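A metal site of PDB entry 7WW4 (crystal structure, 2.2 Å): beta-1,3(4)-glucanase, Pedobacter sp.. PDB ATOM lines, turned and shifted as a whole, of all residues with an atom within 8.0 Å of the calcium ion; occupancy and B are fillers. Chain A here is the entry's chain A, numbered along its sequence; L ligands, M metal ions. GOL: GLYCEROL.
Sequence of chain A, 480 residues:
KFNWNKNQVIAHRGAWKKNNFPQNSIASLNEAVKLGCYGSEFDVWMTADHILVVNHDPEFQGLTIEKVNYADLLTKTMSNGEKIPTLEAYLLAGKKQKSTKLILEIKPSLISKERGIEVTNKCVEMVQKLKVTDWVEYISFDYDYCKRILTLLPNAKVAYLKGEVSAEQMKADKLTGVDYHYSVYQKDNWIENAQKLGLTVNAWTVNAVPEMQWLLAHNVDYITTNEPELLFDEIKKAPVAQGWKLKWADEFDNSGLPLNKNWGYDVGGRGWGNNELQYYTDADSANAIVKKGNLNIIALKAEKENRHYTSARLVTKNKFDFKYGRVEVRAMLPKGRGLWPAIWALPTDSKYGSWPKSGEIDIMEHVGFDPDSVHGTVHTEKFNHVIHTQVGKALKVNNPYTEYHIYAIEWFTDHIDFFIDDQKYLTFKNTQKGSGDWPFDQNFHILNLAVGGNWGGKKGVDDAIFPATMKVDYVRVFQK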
ATOM      1  N   ALA A  11     -19.690  26.631  19.658  1.00  0.00           N
ATOM      2  CA  ALA A  11     -21.021  26.624  20.252  1.00  0.00           C
ATOM      3  C   ALA A  11     -22.069  26.818  19.169  1.00  0.00           C
ATOM      4  O   ALA A  11     -22.232  27.931  18.645  1.00  0.00           O
ATOM      5  CB  ALA A  11     -21.134  27.706  21.321  1.00  0.00           C
ATOM      6  N   HIS A  12     -22.778  25.742  18.821  1.00  0.00           N
ATOM      7  CA  HIS A  12     -23.839  25.791  17.834  1.00  0.00           C
ATOM      8  C   HIS A  12     -24.988  26.671  18.333  1.00  0.00           C
ATOM      9  O   HIS A  12     -25.685  26.297  19.278  1.00  0.00           O
ATOM     10  CB  HIS A  12     -24.335  24.381  17.512  1.00  0.00           C
ATOM     11  CG  HIS A  12     -25.245  24.305  16.325  1.00  0.00           C
ATOM     12  ND1 HIS A  12     -26.530  23.837  16.397  1.00  0.00           N
ATOM     13  CD2 HIS A  12     -25.034  24.629  15.022  1.00  0.00           C
ATOM     14  CE1 HIS A  12     -27.086  23.873  15.198  1.00  0.00           C
ATOM     15  NE2 HIS A  12     -26.202  24.350  14.346  1.00  0.00           N
ATOM     16  N   ARG A  13     -25.160  27.844  17.710  1.00  0.00           N
ATOM     17  CA  ARG A  13     -26.177  28.819  18.104  1.00  0.00           C
ATOM     18  C   ARG A  13     -25.980  29.300  19.546  1.00  0.00           C
ATOM     19  O   ARG A  13     -26.929  29.718  20.206  1.00  0.00           O
ATOM     20  CB  ARG A  13     -27.595  28.264  17.907  1.00  0.00           C
ATOM     21  CG  ARG A  13     -27.821  27.633  16.543  1.00  0.00           C
ATOM     22  CD  ARG A  13     -29.198  27.009  16.440  1.00  0.00           C
ATOM     23  NE  ARG A  13     -29.320  26.183  15.244  1.00  0.00           N
ATOM     24  CZ  ARG A  13     -30.414  25.497  14.916  1.00  0.00           C
ATOM     25  NH1 ARG A  13     -31.475  25.533  15.696  1.00  0.00           N
ATOM     26  NH2 ARG A  13     -30.425  24.774  13.809  1.00  0.00           N
ATOM     27  N   ASN A  24     -29.497  31.321  19.266  1.00  0.00           N
ATOM     28  CA  ASN A  24     -29.058  32.513  18.540  1.00  0.00           C
ATOM     29  C   ASN A  24     -29.465  33.779  19.282  1.00  0.00           C
ATOM     30  O   ASN A  24     -30.064  34.704  18.715  1.00  0.00           O
ATOM     31  CB  ASN A  24     -29.604  32.513  17.105  1.00  0.00           C
ATOM     32  CG  ASN A  24     -28.855  31.557  16.205  1.00  0.00           C
ATOM     33  OD1 ASN A  24     -27.645  31.360  16.344  1.00  0.00           O
ATOM     34  ND2 ASN A  24     -29.572  30.945  15.256  1.00  0.00           N
ATOM     35  N   GLU A  41     -21.201  30.183  17.058  1.00  0.00           N
ATOM     36  CA  GLU A  41     -21.752  30.307  15.720  1.00  0.00           C
ATOM     37  C   GLU A  41     -23.181  30.823  15.782  1.00  0.00           C
ATOM     38  O   GLU A  41     -23.910  30.599  16.753  1.00  0.00           O
ATOM     39  CB  GLU A  41     -21.705  28.963  14.984  1.00  0.00           C
ATOM     40  CG  GLU A  41     -22.813  28.000  15.328  1.00  0.00           C
ATOM     41  CD  GLU A  41     -23.953  28.045  14.325  1.00  0.00           C
ATOM     42  OE1 GLU A  41     -23.676  28.181  13.115  1.00  0.00           O
ATOM     43  OE2 GLU A  41     -25.122  27.930  14.756  1.00  0.00           O
ATOM     44  N   PHE A  42     -23.575  31.532  14.729  1.00  0.00           N
ATOM     45  CA  PHE A  42     -24.894  32.127  14.643  1.00  0.00           C
ATOM     46  C   PHE A  42     -25.268  32.270  13.174  1.00  0.00           C
ATOM     47  O   PHE A  42     -24.406  32.274  12.292  1.00  0.00           O
ATOM     48  CB  PHE A  42     -24.951  33.491  15.356  1.00  0.00           C
ATOM     49  CG  PHE A  42     -23.789  34.393  15.057  1.00  0.00           C
ATOM     50  CD1 PHE A  42     -22.607  34.287  15.780  1.00  0.00           C
ATOM     51  CD2 PHE A  42     -23.867  35.348  14.060  1.00  0.00           C
ATOM     52  CE1 PHE A  42     -21.531  35.114  15.509  1.00  0.00           C
ATOM     53  CE2 PHE A  42     -22.794  36.179  13.780  1.00  0.00           C
ATOM     54  CZ  PHE A  42     -21.628  36.057  14.514  1.00  0.00           C
ATOM     55  N   ASP A  43     -26.572  32.395  12.918  1.00  0.00           N
ATOM     56  CA  ASP A  43     -27.110  32.461  11.563  1.00  0.00           C
ATOM     57  C   ASP A  43     -27.727  33.830  11.340  1.00  0.00           C
ATOM     58  O   ASP A  43     -28.502  34.321  12.168  1.00  0.00           O
ATOM     59  CB  ASP A  43     -28.144  31.356  11.342  1.00  0.00           C
ATOM     60  CG  ASP A  43     -27.707  30.025  11.901  1.00  0.00           C
ATOM     61  OD1 ASP A  43     -28.342  29.529  12.854  1.00  0.00           O
ATOM     62  OD2 ASP A  43     -26.699  29.481  11.397  1.00  0.00           O
ATOM     63  N   VAL A  44     -27.391  34.442  10.206  1.00  0.00           N
ATOM     64  CA  VAL A  44     -27.813  35.804   9.893  1.00  0.00           C
ATOM     65  C   VAL A  44     -28.780  35.778   8.714  1.00  0.00           C
ATOM     66  O   VAL A  44     -28.545  35.077   7.715  1.00  0.00           O
ATOM     67  CB  VAL A  44     -26.609  36.726   9.598  1.00  0.00           C
ATOM     68  CG1 VAL A  44     -25.752  36.158   8.479  1.00  0.00           C
ATOM     69  CG2 VAL A  44     -27.077  38.129   9.262  1.00  0.00           C
ATOM     70  N   ASN A  55     -30.993  34.672  13.434  1.00  0.00           N
ATOM     71  CA  ASN A  55     -32.000  33.636  13.608  1.00  0.00           C
ATOM     72  C   ASN A  55     -31.668  32.495  12.659  1.00  0.00           C
ATOM     73  O   ASN A  55     -31.011  32.709  11.631  1.00  0.00           O
ATOM     74  CB  ASN A  55     -33.421  34.161  13.350  1.00  0.00           C
ATOM     75  CG  ASN A  55     -34.501  33.188  13.771  1.00  0.00           C
ATOM     76  OD1 ASN A  55     -34.462  32.641  14.877  1.00  0.00           O
ATOM     77  ND2 ASN A  55     -35.475  32.973  12.908  1.00  0.00           N
ATOM     78  N   HIS A  56     -32.119  31.287  12.995  1.00  0.00           N
ATOM     79  CA  HIS A  56     -31.845  30.125  12.152  1.00  0.00           C
ATOM     80  C   HIS A  56     -32.964  29.876  11.160  1.00  0.00           C
ATOM     81  O   HIS A  56     -32.730  29.832   9.942  1.00  0.00           O
ATOM     82  CB  HIS A  56     -31.604  28.879  13.015  1.00  0.00           C
ATOM     83  CG  HIS A  56     -31.269  27.661  12.206  1.00  0.00           C
ATOM     84  ND1 HIS A  56     -29.986  27.390  11.773  1.00  0.00           N
ATOM     85  CD2 HIS A  56     -32.043  26.658  11.754  1.00  0.00           C
ATOM     86  CE1 HIS A  56     -29.993  26.263  11.087  1.00  0.00           C
ATOM     87  NE2 HIS A  56     -31.227  25.792  11.059  1.00  0.00           N
ATOM     88  N   ILE A 103     -18.296  32.858  14.889  1.00  0.00           N
ATOM     89  CA  ILE A 103     -18.534  32.098  13.661  1.00  0.00           C
ATOM     90  C   ILE A 103     -19.857  32.572  13.070  1.00  0.00           C
ATOM     91  O   ILE A 103     -20.917  32.407  13.679  1.00  0.00           O
ATOM     92  CB  ILE A 103     -18.550  30.581  13.934  1.00  0.00           C
ATOM     93  CG1 ILE A 103     -17.308  30.170  14.718  1.00  0.00           C
ATOM     94  CG2 ILE A 103     -18.635  29.821  12.623  1.00  0.00           C
ATOM     95  CD1 ILE A 103     -16.001  30.471  14.010  1.00  0.00           C
ATOM     96  N   LEU A 104     -19.791  33.161  11.883  1.00  0.00           N
ATOM     97  CA  LEU A 104     -20.959  33.763  11.238  1.00  0.00           C
ATOM     98  C   LEU A 104     -21.369  32.898  10.058  1.00  0.00           C
ATOM     99  O   LEU A 104     -20.559  32.636   9.170  1.00  0.00           O
ATOM    100  CB  LEU A 104     -20.652  35.192  10.782  1.00  0.00           C
ATOM    101  CG  LEU A 104     -21.813  36.090  10.367  1.00  0.00           C
ATOM    102  CD1 LEU A 104     -21.501  37.531  10.692  1.00  0.00           C
ATOM    103  CD2 LEU A 104     -22.119  35.944   8.894  1.00  0.00           C
ATOM    104  N   GLU A 105     -22.635  32.474  10.048  1.00  0.00           N
ATOM    105  CA  GLU A 105     -23.205  31.720   8.940  1.00  0.00           C
ATOM    106  C   GLU A 105     -24.237  32.575   8.228  1.00  0.00           C
ATOM    107  O   GLU A 105     -25.194  33.039   8.852  1.00  0.00           O
ATOM    108  CB  GLU A 105     -23.829  30.403   9.414  1.00  0.00           C
ATOM    109  CG  GLU A 105     -24.353  29.572   8.257  1.00  0.00           C
ATOM    110  CD  GLU A 105     -24.974  28.273   8.714  1.00  0.00           C
ATOM    111  OE1 GLU A 105     -25.706  27.659   7.907  1.00  0.00           O
ATOM    112  OE2 GLU A 105     -24.736  27.859   9.864  1.00  0.00           O
ATOM    113  N   ILE A 106     -24.051  32.768   6.928  1.00  0.00           N
ATOM    114  CA  ILE A 106     -25.027  33.465   6.097  1.00  0.00           C
ATOM    115  C   ILE A 106     -25.954  32.426   5.494  1.00  0.00           C
ATOM    116  O   ILE A 106     -25.543  31.616   4.659  1.00  0.00           O
ATOM    117  CB  ILE A 106     -24.344  34.295   5.007  1.00  0.00           C
ATOM    118  CG1 ILE A 106     -23.135  35.036   5.575  1.00  0.00           C
ATOM    119  CG2 ILE A 106     -25.324  35.287   4.409  1.00  0.00           C
ATOM    120  CD1 ILE A 106     -22.000  35.181   4.609  1.00  0.00           C
ATOM    121  N   LYS A 107     -27.216  32.441   5.922  1.00  0.00           N
ATOM    122  CA  LYS A 107     -28.179  31.487   5.401  1.00  0.00           C
ATOM    123  C   LYS A 107     -28.506  31.805   3.950  1.00  0.00           C
ATOM    124  O   LYS A 107     -28.644  32.981   3.591  1.00  0.00           O
ATOM    125  CB  LYS A 107     -29.450  31.518   6.250  1.00  0.00           C
ATOM    126  CG  LYS A 107     -29.316  30.837   7.586  1.00  0.00           C
ATOM    127  CD  LYS A 107     -29.188  29.336   7.409  1.00  0.00           C
ATOM    128  CE  LYS A 107     -28.830  28.646   8.712  1.00  0.00           C
ATOM    129  NZ  LYS A 107     -27.903  27.505   8.493  1.00  0.00           N
ATOM    130  N   ILE A 139     -18.915  30.809   7.588  1.00  0.00           N
ATOM    131  CA  ILE A 139     -19.341  29.528   7.049  1.00  0.00           C
ATOM    132  C   ILE A 139     -20.654  29.762   6.302  1.00  0.00           C
ATOM    133  O   ILE A 139     -21.416  30.673   6.640  1.00  0.00           O
ATOM    134  CB  ILE A 139     -19.523  28.457   8.147  1.00  0.00           C
ATOM    135  CG1 ILE A 139     -20.633  28.860   9.115  1.00  0.00           C
ATOM    136  CG2 ILE A 139     -18.225  28.254   8.924  1.00  0.00           C
ATOM    137  CD1 ILE A 139     -20.820  27.897  10.269  1.00  0.00           C
ATOM    138  N   PHE A 141     -23.724  27.737   3.394  1.00  0.00           N
ATOM    139  CA  PHE A 141     -24.176  26.666   2.514  1.00  0.00           C
ATOM    140  C   PHE A 141     -24.049  27.044   1.048  1.00  0.00           C
ATOM    141  O   PHE A 141     -23.847  26.166   0.197  1.00  0.00           O
ATOM    142  CB  PHE A 141     -25.627  26.297   2.828  1.00  0.00           C
ATOM    143  CG  PHE A 141     -25.775  25.228   3.867  1.00  0.00           C
ATOM    144  CD1 PHE A 141     -25.475  23.910   3.581  1.00  0.00           C
ATOM    145  CD2 PHE A 141     -26.229  25.550   5.144  1.00  0.00           C
ATOM    146  CE1 PHE A 141     -25.619  22.927   4.539  1.00  0.00           C
ATOM    147  CE2 PHE A 141     -26.373  24.577   6.106  1.00  0.00           C
ATOM    148  CZ  PHE A 141     -26.066  23.254   5.804  1.00  0.00           C
ATOM    149  N   LEU A 161     -20.419  24.427   3.803  1.00  0.00           N
ATOM    150  CA  LEU A 161     -21.293  23.547   4.559  1.00  0.00           C
ATOM    151  C   LEU A 161     -21.920  22.422   3.738  1.00  0.00           C
ATOM    152  O   LEU A 161     -22.485  21.493   4.319  1.00  0.00           O
ATOM    153  CB  LEU A 161     -22.406  24.357   5.234  1.00  0.00           C
ATOM    154  CG  LEU A 161     -21.953  25.481   6.168  1.00  0.00           C
ATOM    155  CD1 LEU A 161     -23.132  26.304   6.621  1.00  0.00           C
ATOM    156  CD2 LEU A 161     -21.209  24.916   7.371  1.00  0.00           C
ATOM    157  N   ASP A 179     -16.520  22.504   6.491  1.00  0.00           N
ATOM    158  CA  ASP A 179     -17.458  22.413   7.619  1.00  0.00           C
ATOM    159  C   ASP A 179     -18.648  21.561   7.193  1.00  0.00           C
ATOM    160  O   ASP A 179     -19.777  22.035   7.088  1.00  0.00           O
ATOM    161  CB  ASP A 179     -17.891  23.802   8.077  1.00  0.00           C
ATOM    162  CG  ASP A 179     -18.460  23.803   9.487  1.00  0.00           C
ATOM    163  OD1 ASP A 179     -18.644  22.695  10.056  1.00  0.00           O
ATOM    164  OD2 ASP A 179     -18.734  24.895  10.017  1.00  0.00           O
ATOM    165  N   TRP A 204     -20.458  19.594  12.239  1.00  0.00           N
ATOM    166  CA  TRP A 204     -21.566  20.207  12.947  1.00  0.00           C
ATOM    167  C   TRP A 204     -22.661  19.188  13.242  1.00  0.00           C
ATOM    168  O   TRP A 204     -22.671  18.075  12.711  1.00  0.00           O
ATOM    169  CB  TRP A 204     -22.143  21.399  12.169  1.00  0.00           C
ATOM    170  CG  TRP A 204     -22.340  21.184  10.707  1.00  0.00           C
ATOM    171  CD1 TRP A 204     -21.415  21.318   9.715  1.00  0.00           C
ATOM    172  CD2 TRP A 204     -23.570  20.816  10.066  1.00  0.00           C
ATOM    173  NE1 TRP A 204     -21.992  21.060   8.498  1.00  0.00           N
ATOM    174  CE2 TRP A 204     -23.314  20.742   8.679  1.00  0.00           C
ATOM    175  CE3 TRP A 204     -24.857  20.539  10.524  1.00  0.00           C
ATOM    176  CZ2 TRP A 204     -24.291  20.400   7.755  1.00  0.00           C
ATOM    177  CZ3 TRP A 204     -25.835  20.207   9.604  1.00  0.00           C
ATOM    178  CH2 TRP A 204     -25.543  20.139   8.229  1.00  0.00           C
ATOM    179  N   THR A 224     -18.568  21.628  15.941  1.00  0.00           N
ATOM    180  CA  THR A 224     -19.781  22.365  16.258  1.00  0.00           C
ATOM    181  C   THR A 224     -20.750  21.466  17.009  1.00  0.00           C
ATOM    182  O   THR A 224     -21.053  20.354  16.559  1.00  0.00           O
ATOM    183  CB  THR A 224     -20.429  22.904  14.985  1.00  0.00           C
ATOM    184  OG1 THR A 224     -19.428  23.485  14.141  1.00  0.00           O
ATOM    185  CG2 THR A 224     -21.476  23.957  15.318  1.00  0.00           C
HETATM  186  C1  GOL L   1     -25.135  24.039   9.678  1.00  0.00           C
HETATM  187  O1  GOL L   1     -26.326  24.774   9.838  1.00  0.00           O
HETATM  188  C2  GOL L   1     -24.293  24.163  10.934  1.00  0.00           C
HETATM  189  O2  GOL L   1     -25.086  24.687  11.976  1.00  0.00           O
HETATM  190  C3  GOL L   1     -23.127  25.108  10.663  1.00  0.00           C
HETATM  191  O3  GOL L   1     -22.244  25.107  11.772  1.00  0.00           O
HETATM  192 CA    CA M   1     -25.740  27.382  12.100  1.00  0.00          CA
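OD1 of Asp 43 is in hydrogen-bond range of ND1 of His 56 (2.9 Å).
The backbone carbonyl oxygen (O) of Glu 105 sits at hydrogen-bond distance from the backbone NH (N) of Val 44.
The backbone carbonyl oxygen (O) of Glu 41 sits at hydrogen-bond distance from the backbone NH (N) of Arg 13 (3.2 Å).
The backbone NH of Glu 105 is in hydrogen-bond range of the backbone carbonyl oxygen of Phe 42 (2.9 Å).
OE2 of Glu 105 lies close to NZ of Lys 107.
The side-chain carboxylate of Asp 43 sits at hydrogen-bond distance from the side-chain amide nitrogen of Asn 24 (3.0 Å).
The side-chain carboxylate (OD2) of Asp 43 lies close to the side-chain amino group (NZ) of Lys 107 (3.7 Å).
The backbone carbonyl oxygen of Asp 43 sits at hydrogen-bond distance from the backbone NH of Asn 55.
His 12 touches the calcium ion.
Within 4 Å of the calcium ion: His 12, Glu 41, Asp 43 and Glu 105.
The nearest printed residue that does not touch the calcium ion is Lys 107 (4.2 Å).
The side-chain carboxylate (OD2) of Asp 43 binds the calcium ion (2.4 Å).
OE1 of Glu 41 is bound to the calcium ion, 2.4 Å away.
The calcium ion is bound by the side-chain carboxylate (OE2) of Glu 105 (2.5 Å).
O2 of the ligand binds the calcium ion, at 2.8 Å.
The calcium ion is bound by the side-chain carboxylate (OE2) of Glu 41 (2.8 Å).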
